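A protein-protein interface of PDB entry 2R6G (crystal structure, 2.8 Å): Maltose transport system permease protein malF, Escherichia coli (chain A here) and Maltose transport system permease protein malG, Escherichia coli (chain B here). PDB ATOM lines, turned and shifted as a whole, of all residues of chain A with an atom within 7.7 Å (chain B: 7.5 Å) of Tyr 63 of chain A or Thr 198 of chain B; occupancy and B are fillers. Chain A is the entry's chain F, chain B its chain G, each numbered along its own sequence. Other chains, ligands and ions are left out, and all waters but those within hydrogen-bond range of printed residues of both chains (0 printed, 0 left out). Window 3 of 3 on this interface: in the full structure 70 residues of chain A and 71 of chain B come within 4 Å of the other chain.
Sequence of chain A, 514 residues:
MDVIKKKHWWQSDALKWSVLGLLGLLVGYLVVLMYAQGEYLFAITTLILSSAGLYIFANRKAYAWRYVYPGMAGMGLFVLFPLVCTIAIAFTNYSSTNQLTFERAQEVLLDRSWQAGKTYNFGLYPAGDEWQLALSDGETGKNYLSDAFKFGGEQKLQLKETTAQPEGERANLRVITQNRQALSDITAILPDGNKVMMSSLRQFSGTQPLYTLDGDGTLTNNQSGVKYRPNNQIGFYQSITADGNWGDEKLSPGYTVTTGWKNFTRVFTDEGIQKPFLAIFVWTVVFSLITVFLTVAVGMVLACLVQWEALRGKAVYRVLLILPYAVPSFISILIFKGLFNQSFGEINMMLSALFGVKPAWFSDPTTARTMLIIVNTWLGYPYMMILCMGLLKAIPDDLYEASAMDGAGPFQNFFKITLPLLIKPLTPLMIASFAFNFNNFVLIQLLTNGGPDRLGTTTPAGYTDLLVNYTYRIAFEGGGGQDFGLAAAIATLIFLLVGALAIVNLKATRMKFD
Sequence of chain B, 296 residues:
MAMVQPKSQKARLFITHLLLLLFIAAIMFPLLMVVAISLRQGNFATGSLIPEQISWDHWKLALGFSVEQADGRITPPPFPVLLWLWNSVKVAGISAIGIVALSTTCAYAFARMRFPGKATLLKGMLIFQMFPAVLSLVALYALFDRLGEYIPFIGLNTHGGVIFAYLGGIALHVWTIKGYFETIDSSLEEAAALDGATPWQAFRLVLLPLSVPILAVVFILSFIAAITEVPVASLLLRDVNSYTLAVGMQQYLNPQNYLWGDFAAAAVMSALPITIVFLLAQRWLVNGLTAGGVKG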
ATOM      1  N   LYS A  16       4.429   8.509  -1.069  1.00  0.00           N
ATOM      2  CA  LYS A  16       3.031   8.239  -1.411  1.00  0.00           C
ATOM      3  C   LYS A  16       2.226   7.690  -0.231  1.00  0.00           C
ATOM      4  O   LYS A  16       1.006   7.528  -0.328  1.00  0.00           O
ATOM      5  CB  LYS A  16       2.946   7.275  -2.602  1.00  0.00           C
ATOM      6  CG  LYS A  16       3.196   7.920  -3.958  1.00  0.00           C
ATOM      7  CD  LYS A  16       2.933   6.938  -5.091  1.00  0.00           C
ATOM      8  CE  LYS A  16       3.062   7.610  -6.450  1.00  0.00           C
ATOM      9  NZ  LYS A  16       2.813   6.657  -7.567  1.00  0.00           N
ATOM     10  N   ILE A  56      -1.413  -2.995  -5.076  1.00  0.00           N
ATOM     11  CA  ILE A  56      -0.524  -2.920  -6.240  1.00  0.00           C
ATOM     12  C   ILE A  56       0.344  -1.656  -6.277  1.00  0.00           C
ATOM     13  O   ILE A  56       1.430  -1.664  -6.862  1.00  0.00           O
ATOM     14  CB  ILE A  56      -1.289  -3.098  -7.579  1.00  0.00           C
ATOM     15  CG1 ILE A  56      -2.368  -2.023  -7.742  1.00  0.00           C
ATOM     16  CG2 ILE A  56      -1.885  -4.502  -7.669  1.00  0.00           C
ATOM     17  CD1 ILE A  56      -2.790  -1.772  -9.170  1.00  0.00           C
ATOM     18  N   PHE A  57      -0.138  -0.578  -5.658  1.00  0.00           N
ATOM     19  CA  PHE A  57       0.607   0.680  -5.601  1.00  0.00           C
ATOM     20  C   PHE A  57       1.546   0.763  -4.395  1.00  0.00           C
ATOM     21  O   PHE A  57       2.343   1.699  -4.287  1.00  0.00           O
ATOM     22  CB  PHE A  57      -0.349   1.879  -5.606  1.00  0.00           C
ATOM     23  CG  PHE A  57      -1.044   2.101  -6.921  1.00  0.00           C
ATOM     24  CD1 PHE A  57      -2.414   1.896  -7.040  1.00  0.00           C
ATOM     25  CD2 PHE A  57      -0.332   2.519  -8.043  1.00  0.00           C
ATOM     26  CE1 PHE A  57      -3.066   2.098  -8.256  1.00  0.00           C
ATOM     27  CE2 PHE A  57      -0.975   2.723  -9.264  1.00  0.00           C
ATOM     28  CZ  PHE A  57      -2.344   2.513  -9.368  1.00  0.00           C
ATOM     29  N   ALA A  58       1.461  -0.226  -3.505  1.00  0.00           N
ATOM     30  CA  ALA A  58       2.187  -0.201  -2.234  1.00  0.00           C
ATOM     31  C   ALA A  58       3.376  -1.166  -2.182  1.00  0.00           C
ATOM     32  O   ALA A  58       3.983  -1.472  -3.211  1.00  0.00           O
ATOM     33  CB  ALA A  58       1.227  -0.463  -1.075  1.00  0.00           C
ATOM     34  N   ARG A  60       4.291  -4.369  -2.110  1.00  0.00           N
ATOM     35  CA  ARG A  60       4.530  -5.375  -3.137  1.00  0.00           C
ATOM     36  C   ARG A  60       4.485  -4.699  -4.503  1.00  0.00           C
ATOM     37  O   ARG A  60       3.423  -4.256  -4.954  1.00  0.00           O
ATOM     38  CB  ARG A  60       3.505  -6.512  -3.031  1.00  0.00           C
ATOM     39  CG  ARG A  60       3.967  -7.839  -3.627  1.00  0.00           C
ATOM     40  CD  ARG A  60       3.322  -8.107  -4.979  1.00  0.00           C
ATOM     41  NE  ARG A  60       3.880  -9.291  -5.631  1.00  0.00           N
ATOM     42  CZ  ARG A  60       3.350  -9.892  -6.696  1.00  0.00           C
ATOM     43  NH1 ARG A  60       2.229  -9.433  -7.246  1.00  0.00           N
ATOM     44  NH2 ARG A  60       3.945 -10.961  -7.209  1.00  0.00           N
ATOM     45  N   LYS A  61       5.651  -4.600  -5.140  1.00  0.00           N
ATOM     46  CA  LYS A  61       5.770  -3.941  -6.438  1.00  0.00           C
ATOM     47  C   LYS A  61       5.150  -4.784  -7.545  1.00  0.00           C
ATOM     48  O   LYS A  61       5.818  -5.610  -8.176  1.00  0.00           O
ATOM     49  CB  LYS A  61       7.227  -3.582  -6.758  1.00  0.00           C
ATOM     50  CG  LYS A  61       7.822  -2.492  -5.868  1.00  0.00           C
ATOM     51  CD  LYS A  61       7.094  -1.162  -6.025  1.00  0.00           C
ATOM     52  CE  LYS A  61       7.426  -0.214  -4.882  1.00  0.00           C
ATOM     53  NZ  LYS A  61       6.594   1.021  -4.923  1.00  0.00           N
ATOM     54  N   ALA A  62       3.850  -4.578  -7.740  1.00  0.00           N
ATOM     55  CA  ALA A  62       3.110  -5.169  -8.842  1.00  0.00           C
ATOM     56  C   ALA A  62       2.960  -4.106  -9.930  1.00  0.00           C
ATOM     57  O   ALA A  62       1.847  -3.697 -10.280  1.00  0.00           O
ATOM     58  CB  ALA A  62       1.752  -5.662  -8.360  1.00  0.00           C
ATOM     59  N   TYR A  63       4.105  -3.664 -10.449  1.00  0.00           N
ATOM     60  CA  TYR A  63       4.188  -2.544 -11.385  1.00  0.00           C
ATOM     61  C   TYR A  63       3.361  -2.780 -12.644  1.00  0.00           C
ATOM     62  O   TYR A  63       2.720  -1.858 -13.149  1.00  0.00           O
ATOM     63  CB  TYR A  63       5.649  -2.269 -11.749  1.00  0.00           C
ATOM     64  CG  TYR A  63       5.916  -0.890 -12.316  1.00  0.00           C
ATOM     65  CD1 TYR A  63       6.054  -0.695 -13.691  1.00  0.00           C
ATOM     66  CD2 TYR A  63       6.047   0.219 -11.478  1.00  0.00           C
ATOM     67  CE1 TYR A  63       6.306   0.572 -14.219  1.00  0.00           C
ATOM     68  CE2 TYR A  63       6.300   1.493 -11.997  1.00  0.00           C
ATOM     69  CZ  TYR A  63       6.430   1.661 -13.368  1.00  0.00           C
ATOM     70  OH  TYR A  63       6.682   2.915 -13.887  1.00  0.00           O
ATOM     71  N   ALA A  64       3.369  -4.018 -13.131  1.00  0.00           N
ATOM     72  CA  ALA A  64       2.606  -4.397 -14.317  1.00  0.00           C
ATOM     73  C   ALA A  64       1.100  -4.268 -14.092  1.00  0.00           C
ATOM     74  O   ALA A  64       0.357  -3.946 -15.021  1.00  0.00           O
ATOM     75  CB  ALA A  64       2.962  -5.811 -14.748  1.00  0.00           C
ATOM     76  N   TRP A  65       0.662  -4.509 -12.859  1.00  0.00           N
ATOM     77  CA  TRP A  65      -0.757  -4.451 -12.514  1.00  0.00           C
ATOM     78  C   TRP A  65      -1.281  -3.020 -12.382  1.00  0.00           C
ATOM     79  O   TRP A  65      -2.488  -2.791 -12.452  1.00  0.00           O
ATOM     80  CB  TRP A  65      -1.038  -5.254 -11.243  1.00  0.00           C
ATOM     81  CG  TRP A  65      -0.770  -6.722 -11.401  1.00  0.00           C
ATOM     82  CD1 TRP A  65       0.366  -7.390 -11.044  1.00  0.00           C
ATOM     83  CD2 TRP A  65      -1.648  -7.702 -11.969  1.00  0.00           C
ATOM     84  NE1 TRP A  65       0.249  -8.724 -11.347  1.00  0.00           N
ATOM     85  CE2 TRP A  65      -0.977  -8.945 -11.916  1.00  0.00           C
ATOM     86  CE3 TRP A  65      -2.939  -7.652 -12.515  1.00  0.00           C
ATOM     87  CZ2 TRP A  65      -1.552 -10.131 -12.390  1.00  0.00           C
ATOM     88  CZ3 TRP A  65      -3.512  -8.831 -12.986  1.00  0.00           C
ATOM     89  CH2 TRP A  65      -2.815 -10.055 -12.920  1.00  0.00           C
ATOM     90  N   ARG A  66      -0.369  -2.063 -12.206  1.00  0.00           N
ATOM     91  CA  ARG A  66      -0.723  -0.641 -12.121  1.00  0.00           C
ATOM     92  C   ARG A  66      -1.288  -0.118 -13.438  1.00  0.00           C
ATOM     93  O   ARG A  66      -1.970   0.907 -13.467  1.00  0.00           O
ATOM     94  CB  ARG A  66       0.491   0.200 -11.714  1.00  0.00           C
ATOM     95  CG  ARG A  66       1.081  -0.152 -10.359  1.00  0.00           C
ATOM     96  CD  ARG A  66       2.227   0.779 -10.004  1.00  0.00           C
ATOM     97  NE  ARG A  66       2.872   0.397  -8.749  1.00  0.00           N
ATOM     98  CZ  ARG A  66       3.871   1.067  -8.179  1.00  0.00           C
ATOM     99  NH1 ARG A  66       4.353   2.167  -8.743  1.00  0.00           N
ATOM    100  NH2 ARG A  66       4.390   0.636  -7.037  1.00  0.00           N
ATOM    101  N   TYR A  67      -0.994  -0.832 -14.522  1.00  0.00           N
ATOM    102  CA  TYR A  67      -1.450  -0.471 -15.860  1.00  0.00           C
ATOM    103  C   TYR A  67      -2.730  -1.217 -16.234  1.00  0.00           C
ATOM    104  O   TYR A  67      -3.606  -0.664 -16.906  1.00  0.00           O
ATOM    105  CB  TYR A  67      -0.351  -0.763 -16.888  1.00  0.00           C
ATOM    106  CG  TYR A  67       0.874   0.126 -16.780  1.00  0.00           C
ATOM    107  CD1 TYR A  67       1.895  -0.164 -15.873  1.00  0.00           C
ATOM    108  CD2 TYR A  67       1.017   1.249 -17.593  1.00  0.00           C
ATOM    109  CE1 TYR A  67       3.023   0.650 -15.775  1.00  0.00           C
ATOM    110  CE2 TYR A  67       2.140   2.068 -17.503  1.00  0.00           C
ATOM    111  CZ  TYR A  67       3.137   1.763 -16.594  1.00  0.00           C
ATOM    112  OH  TYR A  67       4.249   2.571 -16.502  1.00  0.00           O
ATOM    113  N   VAL A  68      -2.830  -2.470 -15.792  1.00  0.00           N
ATOM    114  CA  VAL A  68      -3.962  -3.336 -16.115  1.00  0.00           C
ATOM    115  C   VAL A  68      -5.185  -3.026 -15.250  1.00  0.00           C
ATOM    116  O   VAL A  68      -6.304  -2.934 -15.758  1.00  0.00           O
ATOM    117  CB  VAL A  68      -3.593  -4.838 -15.965  1.00  0.00           C
ATOM    118  CG1 VAL A  68      -4.706  -5.725 -16.489  1.00  0.00           C
ATOM    119  CG2 VAL A  68      -2.307  -5.151 -16.702  1.00  0.00           C
ATOM    120  N   TYR B 108       0.009  -1.482 -22.968  1.00  0.00           N
ATOM    121  CA  TYR B 108       1.448  -1.392 -22.721  1.00  0.00           C
ATOM    122  C   TYR B 108       1.930  -2.496 -21.789  1.00  0.00           C
ATOM    123  O   TYR B 108       3.038  -3.006 -21.947  1.00  0.00           O
ATOM    124  CB  TYR B 108       1.804  -0.016 -22.149  1.00  0.00           C
ATOM    125  CG  TYR B 108       3.276   0.184 -21.836  1.00  0.00           C
ATOM    126  CD1 TYR B 108       4.231   0.194 -22.849  1.00  0.00           C
ATOM    127  CD2 TYR B 108       3.708   0.384 -20.527  1.00  0.00           C
ATOM    128  CE1 TYR B 108       5.579   0.386 -22.566  1.00  0.00           C
ATOM    129  CE2 TYR B 108       5.055   0.576 -20.234  1.00  0.00           C
ATOM    130  CZ  TYR B 108       5.983   0.575 -21.259  1.00  0.00           C
ATOM    131  OH  TYR B 108       7.318   0.766 -20.984  1.00  0.00           O
ATOM    132  N   ALA B 109       1.086  -2.860 -20.825  1.00  0.00           N
ATOM    133  CA  ALA B 109       1.397  -3.923 -19.878  1.00  0.00           C
ATOM    134  C   ALA B 109       1.307  -5.300 -20.523  1.00  0.00           C
ATOM    135  O   ALA B 109       2.149  -6.160 -20.271  1.00  0.00           O
ATOM    136  CB  ALA B 109       0.490  -3.841 -18.667  1.00  0.00           C
ATOM    137  N   MET B 113       5.277  -6.037 -20.767  1.00  0.00           N
ATOM    138  CA  MET B 113       5.537  -6.575 -19.435  1.00  0.00           C
ATOM    139  C   MET B 113       5.029  -8.001 -19.262  1.00  0.00           C
ATOM    140  O   MET B 113       3.888  -8.315 -19.607  1.00  0.00           O
ATOM    141  CB  MET B 113       4.951  -5.653 -18.365  1.00  0.00           C
ATOM    142  CG  MET B 113       5.780  -4.403 -18.128  1.00  0.00           C
ATOM    143  SD  MET B 113       4.983  -3.224 -17.028  1.00  0.00           S
ATOM    144  CE  MET B 113       4.010  -2.271 -18.179  1.00  0.00           C
ATOM    145  N   PHE B 115       3.825 -10.879 -16.912  1.00  0.00           N
ATOM    146  CA  PHE B 115       3.240 -11.156 -15.600  1.00  0.00           C
ATOM    147  C   PHE B 115       2.347 -12.405 -15.634  1.00  0.00           C
ATOM    148  O   PHE B 115       1.785 -12.729 -16.685  1.00  0.00           O
ATOM    149  CB  PHE B 115       2.484  -9.930 -15.055  1.00  0.00           C
ATOM    150  CG  PHE B 115       1.384  -9.430 -15.955  1.00  0.00           C
ATOM    151  CD1 PHE B 115       0.086  -9.915 -15.826  1.00  0.00           C
ATOM    152  CD2 PHE B 115       1.642  -8.455 -16.914  1.00  0.00           C
ATOM    153  CE1 PHE B 115      -0.935  -9.449 -16.651  1.00  0.00           C
ATOM    154  CE2 PHE B 115       0.629  -7.983 -17.743  1.00  0.00           C
ATOM    155  CZ  PHE B 115      -0.661  -8.480 -17.609  1.00  0.00           C
ATOM    156  N   ALA B 192      15.849   3.587 -24.662  1.00  0.00           N
ATOM    157  CA  ALA B 192      15.265   4.405 -23.605  1.00  0.00           C
ATOM    158  C   ALA B 192      15.690   3.888 -22.235  1.00  0.00           C
ATOM    159  O   ALA B 192      16.099   4.667 -21.373  1.00  0.00           O
ATOM    160  CB  ALA B 192      13.754   4.425 -23.723  1.00  0.00           C
ATOM    161  N   ALA B 193      15.601   2.572 -22.054  1.00  0.00           N
ATOM    162  CA  ALA B 193      15.994   1.925 -20.805  1.00  0.00           C
ATOM    163  C   ALA B 193      17.456   2.211 -20.467  1.00  0.00           C
ATOM    164  O   ALA B 193      17.784   2.509 -19.320  1.00  0.00           O
ATOM    165  CB  ALA B 193      15.741   0.425 -20.883  1.00  0.00           C
ATOM    166  N   ASP B 195      19.055   4.762 -21.520  1.00  0.00           N
ATOM    167  CA  ASP B 195      19.113   6.191 -21.226  1.00  0.00           C
ATOM    168  C   ASP B 195      18.534   6.481 -19.838  1.00  0.00           C
ATOM    169  O   ASP B 195      18.614   7.609 -19.350  1.00  0.00           O
ATOM    170  CB  ASP B 195      18.399   7.011 -22.310  1.00  0.00           C
ATOM    171  CG  ASP B 195      19.276   7.267 -23.536  1.00  0.00           C
ATOM    172  OD1 ASP B 195      20.338   6.620 -23.677  1.00  0.00           O
ATOM    173  OD2 ASP B 195      18.897   8.120 -24.368  1.00  0.00           O
ATOM    174  N   GLY B 196      17.954   5.456 -19.214  1.00  0.00           N
ATOM    175  CA  GLY B 196      17.497   5.536 -17.825  1.00  0.00           C
ATOM    176  C   GLY B 196      16.012   5.770 -17.616  1.00  0.00           C
ATOM    177  O   GLY B 196      15.594   6.185 -16.533  1.00  0.00           O
ATOM    178  N   ALA B 197      15.214   5.497 -18.645  1.00  0.00           N
ATOM    179  CA  ALA B 197      13.769   5.711 -18.587  1.00  0.00           C
ATOM    180  C   ALA B 197      13.050   4.656 -17.751  1.00  0.00           C
ATOM    181  O   ALA B 197      13.321   3.458 -17.880  1.00  0.00           O
ATOM    182  CB  ALA B 197      13.186   5.749 -19.989  1.00  0.00           C
ATOM    183  N   THR B 198      12.146   5.115 -16.884  1.00  0.00           N
ATOM    184  CA  THR B 198      11.205   4.225 -16.208  1.00  0.00           C
ATOM    185  C   THR B 198      10.228   3.712 -17.262  1.00  0.00           C
ATOM    186  O   THR B 198       9.932   4.432 -18.220  1.00  0.00           O
ATOM    187  CB  THR B 198      10.447   4.929 -15.039  1.00  0.00           C
ATOM    188  OG1 THR B 198       9.426   4.062 -14.526  1.00  0.00           O
ATOM    189  CG2 THR B 198       9.790   6.224 -15.483  1.00  0.00           C
ATOM    190  N   PRO B 199       9.754   2.456 -17.123  1.00  0.00           N
ATOM    191  CA  PRO B 199       8.747   1.936 -18.051  1.00  0.00           C
ATOM    192  C   PRO B 199       7.693   2.972 -18.460  1.00  0.00           C
ATOM    193  O   PRO B 199       7.236   2.955 -19.604  1.00  0.00           O
ATOM    194  CB  PRO B 199       8.109   0.799 -17.258  1.00  0.00           C
ATOM    195  CG  PRO B 199       9.220   0.283 -16.408  1.00  0.00           C
ATOM    196  CD  PRO B 199      10.154   1.438 -16.132  1.00  0.00           C
ATOM    197  N   TRP B 200       7.331   3.868 -17.540  1.00  0.00           N
ATOM    198  CA  TRP B 200       6.392   4.956 -17.829  1.00  0.00           C
ATOM    199  C   TRP B 200       6.959   5.986 -18.814  1.00  0.00           C
ATOM    200  O   TRP B 200       6.268   6.400 -19.746  1.00  0.00           O
ATOM    201  CB  TRP B 200       5.942   5.653 -16.538  1.00  0.00           C
ATOM    202  CG  TRP B 200       4.989   6.786 -16.791  1.00  0.00           C
ATOM    203  CD1 TRP B 200       5.298   8.115 -16.881  1.00  0.00           C
ATOM    204  CD2 TRP B 200       3.578   6.686 -17.013  1.00  0.00           C
ATOM    205  NE1 TRP B 200       4.164   8.850 -17.136  1.00  0.00           N
ATOM    206  CE2 TRP B 200       3.094   7.999 -17.221  1.00  0.00           C
ATOM    207  CE3 TRP B 200       2.672   5.617 -17.049  1.00  0.00           C
ATOM    208  CZ2 TRP B 200       1.744   8.271 -17.464  1.00  0.00           C
ATOM    209  CZ3 TRP B 200       1.328   5.888 -17.289  1.00  0.00           C
ATOM    210  CH2 TRP B 200       0.879   7.206 -17.494  1.00  0.00           C
ATOM    211  N   GLN B 201       8.207   6.399 -18.593  1.00  0.00           N
ATOM    212  CA  GLN B 201       8.882   7.373 -19.456  1.00  0.00           C
ATOM    213  C   GLN B 201       9.101   6.834 -20.868  1.00  0.00           C
ATOM    214  O   GLN B 201       9.010   7.582 -21.842  1.00  0.00           O
ATOM    215  CB  GLN B 201      10.216   7.808 -18.843  1.00  0.00           C
ATOM    216  CG  GLN B 201      10.091   8.890 -17.775  1.00  0.00           C
ATOM    217  CD  GLN B 201      11.374   9.097 -16.976  1.00  0.00           C
ATOM    218  OE1 GLN B 201      12.091   8.146 -16.659  1.00  0.00           O
ATOM    219  NE2 GLN B 201      11.660  10.350 -16.642  1.00  0.00           N
ATOM    220  N   ALA B 202       9.390   5.536 -20.962  1.00  0.00           N
ATOM    221  CA  ALA B 202       9.535   4.844 -22.242  1.00  0.00           C
ATOM    222  C   ALA B 202       8.193   4.766 -22.958  1.00  0.00           C
ATOM    223  O   ALA B 202       8.116   4.942 -24.175  1.00  0.00           O
ATOM    224  CB  ALA B 202      10.105   3.451 -22.032  1.00  0.00           C
ATOM    225  N   PHE B 203       7.143   4.504 -22.183  1.00  0.00           N
ATOM    226  CA  PHE B 203       5.772   4.430 -22.680  1.00  0.00           C
ATOM    227  C   PHE B 203       5.283   5.779 -23.198  1.00  0.00           C
ATOM    228  O   PHE B 203       4.752   5.868 -24.306  1.00  0.00           O
ATOM    229  CB  PHE B 203       4.859   3.905 -21.567  1.00  0.00           C
ATOM    230  CG  PHE B 203       3.393   4.160 -21.788  1.00  0.00           C
ATOM    231  CD1 PHE B 203       2.730   5.139 -21.053  1.00  0.00           C
ATOM    232  CD2 PHE B 203       2.670   3.406 -22.707  1.00  0.00           C
ATOM    233  CE1 PHE B 203       1.370   5.375 -21.239  1.00  0.00           C
ATOM    234  CE2 PHE B 203       1.309   3.633 -22.900  1.00  0.00           C
ATOM    235  CZ  PHE B 203       0.659   4.620 -22.164  1.00  0.00           C
ATOM    236  N   ARG B 204       5.480   6.823 -22.399  1.00  0.00           N
ATOM    237  CA  ARG B 204       4.951   8.148 -22.706  1.00  0.00           C
ATOM    238  C   ARG B 204       5.760   8.892 -23.769  1.00  0.00           C
ATOM    239  O   ARG B 204       5.189   9.406 -24.729  1.00  0.00           O
ATOM    240  CB  ARG B 204       4.849   8.998 -21.433  1.00  0.00           C
ATOM    241  CG  ARG B 204       3.896  10.182 -21.558  1.00  0.00           C
ATOM    242  CD  ARG B 204       4.333  11.355 -20.694  1.00  0.00           C
ATOM    243  NE  ARG B 204       3.536  12.551 -20.973  1.00  0.00           N
ATOM    244  CZ  ARG B 204       3.819  13.776 -20.529  1.00  0.00           C
ATOM    245  NH1 ARG B 204       4.894  13.993 -19.777  1.00  0.00           N
ATOM    246  NH2 ARG B 204       3.022  14.790 -20.842  1.00  0.00           N
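OG1 of Thr 198 of chain B sits at hydrogen-bond distance from OH of Tyr 63 of chain A.
OH of Tyr 108 of chain B lies within hydrogen-bond range of O of Pro 199 of chain B (2.6 Å).
OE1 of Gln 201 of chain B lies within hydrogen-bond range of N of Thr 198 of chain B, 3.0 Å away.
Among the printed residues, merely in contact across the chains: Tyr 63 of chain A with Pro 199 of chain B, Tyr 63 of chain A with Trp 200 of chain B, Ala 64 of chain A with Ala 109 of chain B, Ala 64 of chain A with Met 113 of chain B, Ala 64 of chain A with Phe 115 of chain B, Trp 65 of chain A with Phe 115 of chain B, Tyr 67 of chain A with Tyr 108 of chain B, Tyr 67 of chain A with Ala 109 of chain B, Tyr 67 of chain A with Met 113 of chain B, Tyr 67 of chain A with Pro 199 of chain B, Tyr 67 of chain A with Trp 200 of chain B, Val 68 of chain A with Ala 109 of chain B and Val 68 of chain A with Phe 115 of chain B.
Tyr 63 of chain A touches just these residues of chain B: Thr 198 (3.0 Å), Pro 199 (3.5 Å) and Trp 200 (3.8 Å).
Of the printed residues of chain A, Tyr 108 of chain B touches Tyr 67 (3.8 Å).
Of the printed residues of chain A, Ala 109 of chain B touches Ala 64, Tyr 67 and Val 68.
Ala 193 of chain B touches none of the printed residues of chain A.
No residue of chain A comes within 4 Å of Ala 197 of chain B.
Printed residues of chain A within 4 Å of Thr 198 of chain B: Tyr 63 (3.0 Å).
Of the printed residues of chain A, Trp 200 of chain B touches Tyr 63 and Tyr 67.
The nearest residue of chain B that does not touch Tyr 63 of chain A is Met 113 of chain B (4.3 Å).
The nearest printed residue of chain B that does not touch Ala 64 of chain A is Tyr 108 of chain B (7.1 Å).
Hydrophobic or aromatic side chains of chain B that line the printed part of chain A: Tyr 108, Ala 109, Met 113, Phe 115, Pro 199 and Trp 200.
Of the 13 printed residues of chain A, 5 touch a printed residue of chain B.
Printed residues of chain A that touch a printed residue of chain B: Tyr 63, Ala 64, Trp 65, Tyr 67 and Val 68.
Hydrophobic or aromatic side chains of chain A that line the printed part of chain B: Tyr 63, Ala 64, Trp 65, Tyr 67 and Val 68.
Among the printed residues, 14 pairs touch across the chains.
Among the printed residues, no Asp or Glu carboxylate lies within 4 Å of a Lys or Arg side-chain nitrogen of the other chain.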
